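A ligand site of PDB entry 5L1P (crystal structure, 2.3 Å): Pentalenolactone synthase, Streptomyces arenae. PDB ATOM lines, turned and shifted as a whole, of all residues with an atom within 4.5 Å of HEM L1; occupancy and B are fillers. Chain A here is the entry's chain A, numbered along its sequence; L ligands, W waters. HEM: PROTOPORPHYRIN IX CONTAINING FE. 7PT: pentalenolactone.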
ATOM      1  N   MET A  84      23.721  11.024  -4.914  1.00  0.00           N
ATOM      2  CA  MET A  84      23.671  11.560  -6.263  1.00  0.00           C
ATOM      3  C   MET A  84      22.623  10.868  -7.135  1.00  0.00           C
ATOM      4  O   MET A  84      22.637  11.064  -8.355  1.00  0.00           O
ATOM      5  CB  MET A  84      25.051  11.454  -6.911  1.00  0.00           C
ATOM      6  CG  MET A  84      26.143  12.217  -6.128  1.00  0.00           C
ATOM      7  SD  MET A  84      27.816  12.042  -6.813  1.00  0.00           S
ATOM      8  CE  MET A  84      27.623  12.827  -8.414  1.00  0.00           C
ATOM      9  N   HIS A  96      17.504  11.347 -10.926  1.00  0.00           N
ATOM     10  CA  HIS A  96      18.512  12.383 -11.108  1.00  0.00           C
ATOM     11  C   HIS A  96      17.908  13.654 -11.709  1.00  0.00           C
ATOM     12  O   HIS A  96      18.273  14.767 -11.309  1.00  0.00           O
ATOM     13  CB  HIS A  96      19.639  11.865 -11.986  1.00  0.00           C
ATOM     14  CG  HIS A  96      20.737  12.864 -12.186  1.00  0.00           C
ATOM     15  ND1 HIS A  96      21.030  13.404 -13.421  1.00  0.00           N
ATOM     16  CD2 HIS A  96      21.579  13.445 -11.296  1.00  0.00           C
ATOM     17  CE1 HIS A  96      22.019  14.273 -13.286  1.00  0.00           C
ATOM     18  NE2 HIS A  96      22.365  14.317 -12.006  1.00  0.00           N
ATOM     19  N   MET A  99      16.160  15.430  -8.985  1.00  0.00           N
ATOM     20  CA  MET A  99      17.112  15.995  -8.040  1.00  0.00           C
ATOM     21  C   MET A  99      17.677  17.323  -8.529  1.00  0.00           C
ATOM     22  O   MET A  99      17.744  18.297  -7.765  1.00  0.00           O
ATOM     23  CB  MET A  99      18.240  14.994  -7.801  1.00  0.00           C
ATOM     24  CG  MET A  99      19.427  15.587  -7.092  1.00  0.00           C
ATOM     25  SD  MET A  99      20.570  14.315  -6.564  1.00  0.00           S
ATOM     26  CE  MET A  99      21.795  15.307  -5.707  1.00  0.00           C
ATOM     27  N   ARG A 100      18.094  17.373  -9.797  1.00  0.00           N
ATOM     28  CA  ARG A 100      18.606  18.623 -10.349  1.00  0.00           C
ATOM     29  C   ARG A 100      17.494  19.656 -10.463  1.00  0.00           C
ATOM     30  O   ARG A 100      17.713  20.843 -10.184  1.00  0.00           O
ATOM     31  CB  ARG A 100      19.257  18.381 -11.706  1.00  0.00           C
ATOM     32  CG  ARG A 100      20.614  17.703 -11.579  1.00  0.00           C
ATOM     33  CD  ARG A 100      21.304  17.613 -12.905  1.00  0.00           C
ATOM     34  NE  ARG A 100      21.867  18.884 -13.359  1.00  0.00           N
ATOM     35  CZ  ARG A 100      23.012  19.405 -12.923  1.00  0.00           C
ATOM     36  NH1 ARG A 100      23.730  18.799 -11.992  1.00  0.00           N
ATOM     37  NH2 ARG A 100      23.442  20.556 -13.435  1.00  0.00           N
ATOM     38  N   LEU A 103      16.970  21.190  -7.017  1.00  0.00           N
ATOM     39  CA  LEU A 103      18.086  21.886  -6.362  1.00  0.00           C
ATOM     40  C   LEU A 103      18.554  23.124  -7.119  1.00  0.00           C
ATOM     41  O   LEU A 103      18.951  24.100  -6.485  1.00  0.00           O
ATOM     42  CB  LEU A 103      19.275  20.938  -6.152  1.00  0.00           C
ATOM     43  CG  LEU A 103      19.102  19.847  -5.074  1.00  0.00           C
ATOM     44  CD1 LEU A 103      20.297  18.911  -5.051  1.00  0.00           C
ATOM     45  CD2 LEU A 103      18.876  20.479  -3.708  1.00  0.00           C
ATOM     46  N   PHE A 107      19.477  27.896  -6.000  1.00  0.00           N
ATOM     47  CA  PHE A 107      20.637  28.759  -6.134  1.00  0.00           C
ATOM     48  C   PHE A 107      20.293  29.897  -7.086  1.00  0.00           C
ATOM     49  O   PHE A 107      20.935  30.061  -8.135  1.00  0.00           O
ATOM     50  CB  PHE A 107      21.843  27.934  -6.579  1.00  0.00           C
ATOM     51  CG  PHE A 107      22.246  26.876  -5.573  1.00  0.00           C
ATOM     52  CD1 PHE A 107      21.581  25.650  -5.524  1.00  0.00           C
ATOM     53  CD2 PHE A 107      23.294  27.110  -4.654  1.00  0.00           C
ATOM     54  CE1 PHE A 107      21.939  24.668  -4.572  1.00  0.00           C
ATOM     55  CE2 PHE A 107      23.662  26.142  -3.717  1.00  0.00           C
ATOM     56  CZ  PHE A 107      22.982  24.923  -3.664  1.00  0.00           C
ATOM     57  N   LEU A 155      22.412  28.285   4.030  1.00  0.00           N
ATOM     58  CA  LEU A 155      21.588  27.532   3.082  1.00  0.00           C
ATOM     59  C   LEU A 155      20.494  26.754   3.798  1.00  0.00           C
ATOM     60  O   LEU A 155      19.338  26.752   3.361  1.00  0.00           O
ATOM     61  CB  LEU A 155      22.450  26.585   2.247  1.00  0.00           C
ATOM     62  CG  LEU A 155      23.370  27.239   1.233  1.00  0.00           C
ATOM     63  CD1 LEU A 155      24.250  26.196   0.555  1.00  0.00           C
ATOM     64  CD2 LEU A 155      22.547  28.011   0.212  1.00  0.00           C
ATOM     65  N   PHE A 235      27.968  17.758   0.359  1.00  0.00           N
ATOM     66  CA  PHE A 235      28.726  18.306  -0.757  1.00  0.00           C
ATOM     67  C   PHE A 235      28.965  19.828  -0.632  1.00  0.00           C
ATOM     68  O   PHE A 235      29.811  20.372  -1.357  1.00  0.00           O
ATOM     69  CB  PHE A 235      28.018  18.024  -2.110  1.00  0.00           C
ATOM     70  CG  PHE A 235      27.697  16.541  -2.341  1.00  0.00           C
ATOM     71  CD1 PHE A 235      28.460  15.539  -1.764  1.00  0.00           C
ATOM     72  CD2 PHE A 235      26.611  16.178  -3.129  1.00  0.00           C
ATOM     73  CE1 PHE A 235      28.165  14.189  -1.978  1.00  0.00           C
ATOM     74  CE2 PHE A 235      26.292  14.836  -3.346  1.00  0.00           C
ATOM     75  CZ  PHE A 235      27.070  13.836  -2.771  1.00  0.00           C
ATOM     76  N   GLY A 236      28.256  20.508   0.265  1.00  0.00           N
ATOM     77  CA  GLY A 236      28.234  21.963   0.220  1.00  0.00           C
ATOM     78  C   GLY A 236      29.392  22.673   0.885  1.00  0.00           C
ATOM     79  O   GLY A 236      29.504  23.900   0.715  1.00  0.00           O
ATOM     80  N   THR A 239      34.516  20.354  -0.138  1.00  0.00           N
ATOM     81  CA  THR A 239      35.325  20.653  -1.320  1.00  0.00           C
ATOM     82  C   THR A 239      35.734  22.120  -1.349  1.00  0.00           C
ATOM     83  O   THR A 239      36.864  22.443  -1.756  1.00  0.00           O
ATOM     84  CB  THR A 239      34.582  20.306  -2.614  1.00  0.00           C
ATOM     85  OG1 THR A 239      33.356  21.038  -2.664  1.00  0.00           O
ATOM     86  CG2 THR A 239      34.300  18.806  -2.715  1.00  0.00           C
ATOM     87  N   THR A 240      34.839  23.019  -0.928  1.00  0.00           N
ATOM     88  CA  THR A 240      35.180  24.440  -0.919  1.00  0.00           C
ATOM     89  C   THR A 240      36.307  24.732   0.077  1.00  0.00           C
ATOM     90  O   THR A 240      37.202  25.526  -0.205  1.00  0.00           O
ATOM     91  CB  THR A 240      33.948  25.279  -0.570  1.00  0.00           C
ATOM     92  OG1 THR A 240      32.852  24.893  -1.411  1.00  0.00           O
ATOM     93  CG2 THR A 240      34.242  26.743  -0.858  1.00  0.00           C
ATOM     94  N   ARG A 243      39.462  23.735  -1.536  1.00  0.00           N
ATOM     95  CA  ARG A 243      39.890  24.705  -2.551  1.00  0.00           C
ATOM     96  C   ARG A 243      40.468  25.969  -1.920  1.00  0.00           C
ATOM     97  O   ARG A 243      41.335  26.609  -2.524  1.00  0.00           O
ATOM     98  CB  ARG A 243      38.729  25.033  -3.500  1.00  0.00           C
ATOM     99  CG  ARG A 243      38.328  23.868  -4.407  1.00  0.00           C
ATOM    100  CD  ARG A 243      39.532  22.958  -4.720  1.00  0.00           C
ATOM    101  NE  ARG A 243      39.173  21.790  -5.519  1.00  0.00           N
ATOM    102  CZ  ARG A 243      38.619  20.687  -5.025  1.00  0.00           C
ATOM    103  NH1 ARG A 243      38.347  20.590  -3.734  1.00  0.00           N
ATOM    104  NH2 ARG A 243      38.331  19.672  -5.832  1.00  0.00           N
ATOM    105  N   LEU A 276      41.022  26.832  -9.229  1.00  0.00           N
ATOM    106  CA  LEU A 276      40.213  25.652  -9.500  1.00  0.00           C
ATOM    107  C   LEU A 276      40.878  24.741 -10.519  1.00  0.00           C
ATOM    108  O   LEU A 276      40.887  23.510 -10.360  1.00  0.00           O
ATOM    109  CB  LEU A 276      38.831  26.080  -9.986  1.00  0.00           C
ATOM    110  CG  LEU A 276      37.990  26.697  -8.871  1.00  0.00           C
ATOM    111  CD1 LEU A 276      36.823  27.479  -9.484  1.00  0.00           C
ATOM    112  CD2 LEU A 276      37.472  25.604  -7.920  1.00  0.00           C
ATOM    113  N   ILE A 289      36.507  11.644 -11.929  1.00  0.00           N
ATOM    114  CA  ILE A 289      35.060  11.454 -11.943  1.00  0.00           C
ATOM    115  C   ILE A 289      34.788  10.020 -12.432  1.00  0.00           C
ATOM    116  O   ILE A 289      35.198   9.688 -13.561  1.00  0.00           O
ATOM    117  CB  ILE A 289      34.372  12.485 -12.828  1.00  0.00           C
ATOM    118  CG1 ILE A 289      34.418  13.872 -12.164  1.00  0.00           C
ATOM    119  CG2 ILE A 289      32.936  12.055 -13.169  1.00  0.00           C
ATOM    120  CD1 ILE A 289      33.784  14.990 -13.036  1.00  0.00           C
ATOM    121  N   ARG A 291      32.609   6.743 -13.851  1.00  0.00           N
ATOM    122  CA  ARG A 291      31.424   6.453 -14.658  1.00  0.00           C
ATOM    123  C   ARG A 291      31.472   4.998 -15.085  1.00  0.00           C
ATOM    124  O   ARG A 291      32.521   4.345 -15.036  1.00  0.00           O
ATOM    125  CB  ARG A 291      31.336   7.317 -15.923  1.00  0.00           C
ATOM    126  CG  ARG A 291      31.180   8.805 -15.715  1.00  0.00           C
ATOM    127  CD  ARG A 291      29.784   9.166 -15.256  1.00  0.00           C
ATOM    128  NE  ARG A 291      29.607  10.618 -15.216  1.00  0.00           N
ATOM    129  CZ  ARG A 291      29.629  11.367 -14.118  1.00  0.00           C
ATOM    130  NH1 ARG A 291      29.817  10.811 -12.914  1.00  0.00           N
ATOM    131  NH2 ARG A 291      29.463  12.682 -14.223  1.00  0.00           N
ATOM    132  N   ILE A 314      39.629  14.695 -14.501  1.00  0.00           N
ATOM    133  CA  ILE A 314      39.426  16.134 -14.705  1.00  0.00           C
ATOM    134  C   ILE A 314      40.629  16.932 -14.227  1.00  0.00           C
ATOM    135  O   ILE A 314      40.874  18.035 -14.715  1.00  0.00           O
ATOM    136  CB  ILE A 314      38.134  16.603 -14.021  1.00  0.00           C
ATOM    137  CG1 ILE A 314      38.202  16.367 -12.500  1.00  0.00           C
ATOM    138  CG2 ILE A 314      36.915  15.932 -14.657  1.00  0.00           C
ATOM    139  CD1 ILE A 314      37.005  16.945 -11.726  1.00  0.00           C
ATOM    140  N   ALA A 342      36.961  21.475 -13.434  1.00  0.00           N
ATOM    141  CA  ALA A 342      36.983  21.197 -12.000  1.00  0.00           C
ATOM    142  C   ALA A 342      35.592  21.103 -11.387  1.00  0.00           C
ATOM    143  O   ALA A 342      35.460  20.536 -10.293  1.00  0.00           O
ATOM    144  CB  ALA A 342      37.813  22.250 -11.254  1.00  0.00           C
ATOM    145  N   PHE A 343      34.561  21.663 -12.030  1.00  0.00           N
ATOM    146  CA  PHE A 343      33.183  21.488 -11.597  1.00  0.00           C
ATOM    147  C   PHE A 343      32.464  20.419 -12.404  1.00  0.00           C
ATOM    148  O   PHE A 343      31.228  20.348 -12.364  1.00  0.00           O
ATOM    149  CB  PHE A 343      32.401  22.795 -11.692  1.00  0.00           C
ATOM    150  CG  PHE A 343      32.771  23.832 -10.648  1.00  0.00           C
ATOM    151  CD1 PHE A 343      32.607  23.576  -9.301  1.00  0.00           C
ATOM    152  CD2 PHE A 343      33.235  25.098 -11.025  1.00  0.00           C
ATOM    153  CE1 PHE A 343      32.919  24.549  -8.346  1.00  0.00           C
ATOM    154  CE2 PHE A 343      33.558  26.075 -10.085  1.00  0.00           C
ATOM    155  CZ  PHE A 343      33.397  25.799  -8.742  1.00  0.00           C
ATOM    156  N   GLY A 344      33.200  19.616 -13.157  1.00  0.00           N
ATOM    157  CA  GLY A 344      32.565  18.659 -14.023  1.00  0.00           C
ATOM    158  C   GLY A 344      32.014  19.301 -15.281  1.00  0.00           C
ATOM    159  O   GLY A 344      32.390  20.415 -15.676  1.00  0.00           O
ATOM    160  N   ALA A 347      25.777  16.245 -17.787  1.00  0.00           N
ATOM    161  CA  ALA A 347      24.532  16.027 -17.054  1.00  0.00           C
ATOM    162  C   ALA A 347      24.680  16.275 -15.551  1.00  0.00           C
ATOM    163  O   ALA A 347      23.703  16.642 -14.881  1.00  0.00           O
ATOM    164  CB  ALA A 347      24.025  14.608 -17.321  1.00  0.00           C
ATOM    165  N   ARG A 348      25.865  16.075 -14.990  1.00  0.00           N
ATOM    166  CA  ARG A 348      26.032  16.243 -13.544  1.00  0.00           C
ATOM    167  C   ARG A 348      26.896  17.456 -13.182  1.00  0.00           C
ATOM    168  O   ARG A 348      27.443  17.514 -12.079  1.00  0.00           O
ATOM    169  CB  ARG A 348      26.602  14.966 -12.933  1.00  0.00           C
ATOM    170  CG  ARG A 348      25.634  13.770 -13.047  1.00  0.00           C
ATOM    171  CD  ARG A 348      26.177  12.539 -12.367  1.00  0.00           C
ATOM    172  NE  ARG A 348      25.191  11.470 -12.280  1.00  0.00           N
ATOM    173  CZ  ARG A 348      24.307  11.347 -11.292  1.00  0.00           C
ATOM    174  NH1 ARG A 348      24.265  12.250 -10.307  1.00  0.00           N
ATOM    175  NH2 ARG A 348      23.449  10.328 -11.287  1.00  0.00           N
ATOM    176  N   HIS A 349      26.996  18.429 -14.103  1.00  0.00           N
ATOM    177  CA  HIS A 349      27.698  19.690 -13.842  1.00  0.00           C
ATOM    178  C   HIS A 349      27.314  20.273 -12.484  1.00  0.00           C
ATOM    179  O   HIS A 349      26.134  20.463 -12.188  1.00  0.00           O
ATOM    180  CB  HIS A 349      27.385  20.686 -14.963  1.00  0.00           C
ATOM    181  CG  HIS A 349      28.360  21.800 -15.085  1.00  0.00           C
ATOM    182  ND1 HIS A 349      28.216  22.824 -16.001  1.00  0.00           N
ATOM    183  CD2 HIS A 349      29.503  22.076 -14.404  1.00  0.00           C
ATOM    184  CE1 HIS A 349      29.227  23.670 -15.895  1.00  0.00           C
ATOM    185  NE2 HIS A 349      30.016  23.239 -14.926  1.00  0.00           N
ATOM    186  N   CYS A 350      28.335  20.553 -11.677  1.00  0.00           N
ATOM    187  CA  CYS A 350      28.183  20.953 -10.276  1.00  0.00           C
ATOM    188  C   CYS A 350      27.094  22.011 -10.094  1.00  0.00           C
ATOM    189  O   CYS A 350      27.106  23.053 -10.754  1.00  0.00           O
ATOM    190  CB  CYS A 350      29.512  21.506  -9.766  1.00  0.00           C
ATOM    191  SG  CYS A 350      29.382  22.432  -8.196  1.00  0.00           S
ATOM    192  N   ILE A 351      26.165  21.741  -9.180  1.00  0.00           N
ATOM    193  CA  ILE A 351      25.047  22.670  -8.977  1.00  0.00           C
ATOM    194  C   ILE A 351      25.426  23.841  -8.058  1.00  0.00           C
ATOM    195  O   ILE A 351      24.858  24.935  -8.185  1.00  0.00           O
ATOM    196  CB  ILE A 351      23.815  21.914  -8.441  1.00  0.00           C
ATOM    197  CG1 ILE A 351      23.257  20.969  -9.504  1.00  0.00           C
ATOM    198  CG2 ILE A 351      22.706  22.882  -8.038  1.00  0.00           C
ATOM    199  CD1 ILE A 351      22.223  20.017  -8.931  1.00  0.00           C
ATOM    200  N   GLY A 352      26.363  23.651  -7.131  1.00  0.00           N
ATOM    201  CA  GLY A 352      26.748  24.774  -6.285  1.00  0.00           C
ATOM    202  C   GLY A 352      27.897  25.620  -6.810  1.00  0.00           C
ATOM    203  O   GLY A 352      28.517  26.390  -6.057  1.00  0.00           O
ATOM    204  N   LEU A 355      27.913  29.445  -6.274  1.00  0.00           N
ATOM    205  CA  LEU A 355      28.105  29.764  -4.859  1.00  0.00           C
ATOM    206  C   LEU A 355      29.573  29.567  -4.466  1.00  0.00           C
ATOM    207  O   LEU A 355      30.167  30.441  -3.808  1.00  0.00           O
ATOM    208  CB  LEU A 355      27.162  28.891  -4.013  1.00  0.00           C
ATOM    209  CG  LEU A 355      27.142  29.124  -2.489  1.00  0.00           C
ATOM    210  CD1 LEU A 355      27.046  30.597  -2.146  1.00  0.00           C
ATOM    211  CD2 LEU A 355      26.026  28.328  -1.809  1.00  0.00           C
ATOM    212  N   ALA A 356      30.178  28.445  -4.875  1.00  0.00           N
ATOM    213  CA  ALA A 356      31.570  28.185  -4.531  1.00  0.00           C
ATOM    214  C   ALA A 356      32.487  29.279  -5.067  1.00  0.00           C
ATOM    215  O   ALA A 356      33.406  29.729  -4.373  1.00  0.00           O
ATOM    216  CB  ALA A 356      32.008  26.820  -5.083  1.00  0.00           C
ATOM    217  N   LEU A 360      35.038  31.586  -2.943  1.00  0.00           N
ATOM    218  CA  LEU A 360      36.464  31.639  -3.227  1.00  0.00           C
ATOM    219  C   LEU A 360      36.878  33.052  -3.604  1.00  0.00           C
ATOM    220  O   LEU A 360      37.936  33.532  -3.170  1.00  0.00           O
ATOM    221  CB  LEU A 360      36.798  30.652  -4.344  1.00  0.00           C
ATOM    222  CG  LEU A 360      36.707  29.189  -3.909  1.00  0.00           C
ATOM    223  CD1 LEU A 360      36.786  28.221  -5.090  1.00  0.00           C
ATOM    224  CD2 LEU A 360      37.779  28.853  -2.863  1.00  0.00           C
HETATM  225  CHA HEM L   1      28.707  17.796  -8.412  1.00  0.00           C
HETATM  226  CHB HEM L   1      33.037  19.852  -7.726  1.00  0.00           C
HETATM  227  CHC HEM L   1      31.141  22.945  -4.496  1.00  0.00           C
HETATM  228  CHD HEM L   1      26.920  20.625  -4.869  1.00  0.00           C
HETATM  229  C1A HEM L   1      30.013  18.131  -8.573  1.00  0.00           C
HETATM  230  C2A HEM L   1      30.934  17.572  -9.546  1.00  0.00           C
HETATM  231  C3A HEM L   1      32.133  18.138  -9.341  1.00  0.00           C
HETATM  232  C4A HEM L   1      32.014  19.073  -8.239  1.00  0.00           C
HETATM  233  CMA HEM L   1      33.427  17.863 -10.140  1.00  0.00           C
HETATM  234  CAA HEM L   1      30.584  16.514 -10.632  1.00  0.00           C
HETATM  235  CBA HEM L   1      30.667  15.083 -10.079  1.00  0.00           C
HETATM  236  CGA HEM L   1      30.247  14.109 -11.171  1.00  0.00           C
HETATM  237  O1A HEM L   1      30.050  14.565 -12.331  1.00  0.00           O
HETATM  238  O2A HEM L   1      30.119  12.880 -10.884  1.00  0.00           O
HETATM  239  C1B HEM L   1      32.916  20.857  -6.801  1.00  0.00           C
HETATM  240  C2B HEM L   1      33.980  21.729  -6.323  1.00  0.00           C
HETATM  241  C3B HEM L   1      33.430  22.550  -5.418  1.00  0.00           C
HETATM  242  C4B HEM L   1      32.025  22.263  -5.309  1.00  0.00           C
HETATM  243  CMB HEM L   1      35.464  21.645  -6.780  1.00  0.00           C
HETATM  244  CAB HEM L   1      34.052  23.708  -4.600  1.00  0.00           C
HETATM  245  CBB HEM L   1      35.036  24.459  -5.110  1.00  0.00           C
HETATM  246  C1C HEM L   1      29.811  22.643  -4.305  1.00  0.00           C
HETATM  247  C2C HEM L   1      28.857  23.366  -3.484  1.00  0.00           C
HETATM  248  C3C HEM L   1      27.681  22.707  -3.605  1.00  0.00           C
HETATM  249  C4C HEM L   1      27.878  21.560  -4.482  1.00  0.00           C
HETATM  250  CMC HEM L   1      29.183  24.672  -2.675  1.00  0.00           C
HETATM  251  CAC HEM L   1      26.288  22.987  -2.972  1.00  0.00           C
HETATM  252  CBC HEM L   1      26.032  23.866  -2.004  1.00  0.00           C
HETATM  253  C1D HEM L   1      27.041  19.646  -5.825  1.00  0.00           C
HETATM  254  C2D HEM L   1      26.027  18.670  -6.189  1.00  0.00           C
HETATM  255  C3D HEM L   1      26.527  17.884  -7.161  1.00  0.00           C
HETATM  256  C4D HEM L   1      27.869  18.326  -7.448  1.00  0.00           C
HETATM  257  CMD HEM L   1      24.624  18.554  -5.578  1.00  0.00           C
HETATM  258  CAD HEM L   1      25.804  16.725  -7.865  1.00  0.00           C
HETATM  259  CBD HEM L   1      25.427  17.122  -9.299  1.00  0.00           C
HETATM  260  CGD HEM L   1      24.738  15.959  -9.951  1.00  0.00           C
HETATM  261  O1D HEM L   1      23.801  16.198 -10.748  1.00  0.00           O
HETATM  262  O2D HEM L   1      25.084  14.773  -9.685  1.00  0.00           O
HETATM  263  NA  HEM L   1      30.702  19.047  -7.792  1.00  0.00           N
HETATM  264  NB  HEM L   1      31.745  21.205  -6.159  1.00  0.00           N
HETATM  265  NC  HEM L   1      29.190  21.560  -4.896  1.00  0.00           N
HETATM  266  ND  HEM L   1      28.152  19.398  -6.618  1.00  0.00           N
HETATM  267 FE   HEM L   1      29.872  20.532  -6.607  1.00  0.00          FE
HETATM  268  C1  7PT L   2      31.706  16.282  -6.201  1.00  0.00           C
HETATM  269  O1  7PT L   2      33.534  13.530  -8.707  1.00  0.00           O
HETATM  270  C2  7PT L   2      31.168  15.020  -5.842  1.00  0.00           C
HETATM  271  C3  7PT L   2      32.058  14.014  -5.932  1.00  0.00           C
HETATM  272  C4  7PT L   2      33.332  14.503  -6.311  1.00  0.00           C
HETATM  273  C5  7PT L   2      34.242  14.781  -5.086  1.00  0.00           C
HETATM  274  C15 7PT L   2      29.687  14.812  -5.472  1.00  0.00           C
HETATM  275  C14 7PT L   2      31.764  17.187  -4.969  1.00  0.00           C
HETATM  276  C7  7PT L   2      34.239  16.631  -6.438  1.00  0.00           C
HETATM  277  C12 7PT L   2      35.287  13.642  -5.001  1.00  0.00           C
HETATM  278  C10 7PT L   2      34.893  14.077  -8.446  1.00  0.00           C
HETATM  279  C13 7PT L   2      36.023  16.484  -4.825  1.00  0.00           C
HETATM  280  C11 7PT L   2      34.280  12.320  -6.774  1.00  0.00           C
HETATM  281  C6  7PT L   2      34.897  16.012  -5.415  1.00  0.00           C
HETATM  282  C8  7PT L   2      33.074  15.902  -6.867  1.00  0.00           C
HETATM  283  C9  7PT L   2      33.998  13.566  -7.350  1.00  0.00           C
HETATM  284  O4  7PT L   2      36.566  15.930  -3.848  1.00  0.00           O
HETATM  285  O2  7PT L   2      33.946  11.292  -7.360  1.00  0.00           O
HETATM  286  O5  7PT L   2      36.575  17.547  -5.201  1.00  0.00           O
HETATM  287  O3  7PT L   2      34.835  12.343  -5.518  1.00  0.00           O
HETATM  288  O   HOH W   1      31.062  19.727  -3.339  1.00  0.00           O
HETATM  289  O   HOH W   2      30.024  16.356 -14.143  1.00  0.00           O
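A ring nitrogen (NE2) of His 96 sits close to the guanidinium group (NH1) of Arg 348 (3.3 Å).
The backbone NH (N) of Cys 350 is in hydrogen-bond range of the backbone carbonyl oxygen (O) of Phe 343.
The guanidinium group (NE) of Arg 100 lies close to the backbone carbonyl oxygen (O) of Ala 347.
O of Thr 239 sits at hydrogen-bond distance from NH1 of Arg 243 (3.1 Å).
O of Met 84 lies within hydrogen-bond range of NH1 of Arg 348 (2.8 Å).
The guanidinium group of Arg 100 is in hydrogen-bond range of the backbone carbonyl oxygen of His 349 (2.9 Å).
SG of Cys 350 sits close to N of Gly 352 (3.4 Å).
Water W1 lies within hydrogen-bond range of O of Phe 235 and OG1 of Thr 239.
The guanidinium group (NH2) of Arg 291 is in salt-bridge range of an oxygen (O1A) of HEM L1 (2.7 Å).
An oxygen (O2D) of HEM L1 lies within salt-bridge range of the guanidinium group of Arg 348.
NH2 of Arg 243 lies within salt-bridge range of O5 of 7PT L2, at 2.8 Å.
O1D of HEM L1 is in hydrogen-bond range of NE2 of His 96 (2.7 Å).
The side-chain sulfur (SG) of Cys 350 is bound to an iron atom (FE) of HEM L1, 2.5 Å away.
NH1 of Arg 100 lies within salt-bridge range of O1D of HEM L1, at 2.9 Å.
Residues that only touch HEM L1: Met 84, Phe 107, Leu 155, Phe 235, Gly 236, Thr 239, Thr 240, Arg 243, Leu 276, Ile 289, Ala 342, Phe 343, Gly 344, Gly 352 and Ala 356.
Hydrophobic or aromatic side chains that line HEM L1: Met 84, His 96, Phe 107, Leu 155, Phe 235, Leu 276, Ile 289, Phe 343 and Ala 356.
20 residues have an atom within 4 Å of HEM L1: Met 84, His 96, Arg 100, Phe 107, Leu 155, Phe 235, Gly 236, Thr 239, Thr 240, Arg 243, Leu 276, Ile 289, Arg 291, Ala 342, Phe 343, Gly 344, Arg 348, Cys 350, Gly 352 and Ala 356.
Along chain A the residues within 4 Å of HEM L1 span positions 84 to 356.
The nearest printed residue that does not touch HEM L1 is Ile 351 (4.0002 Å).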
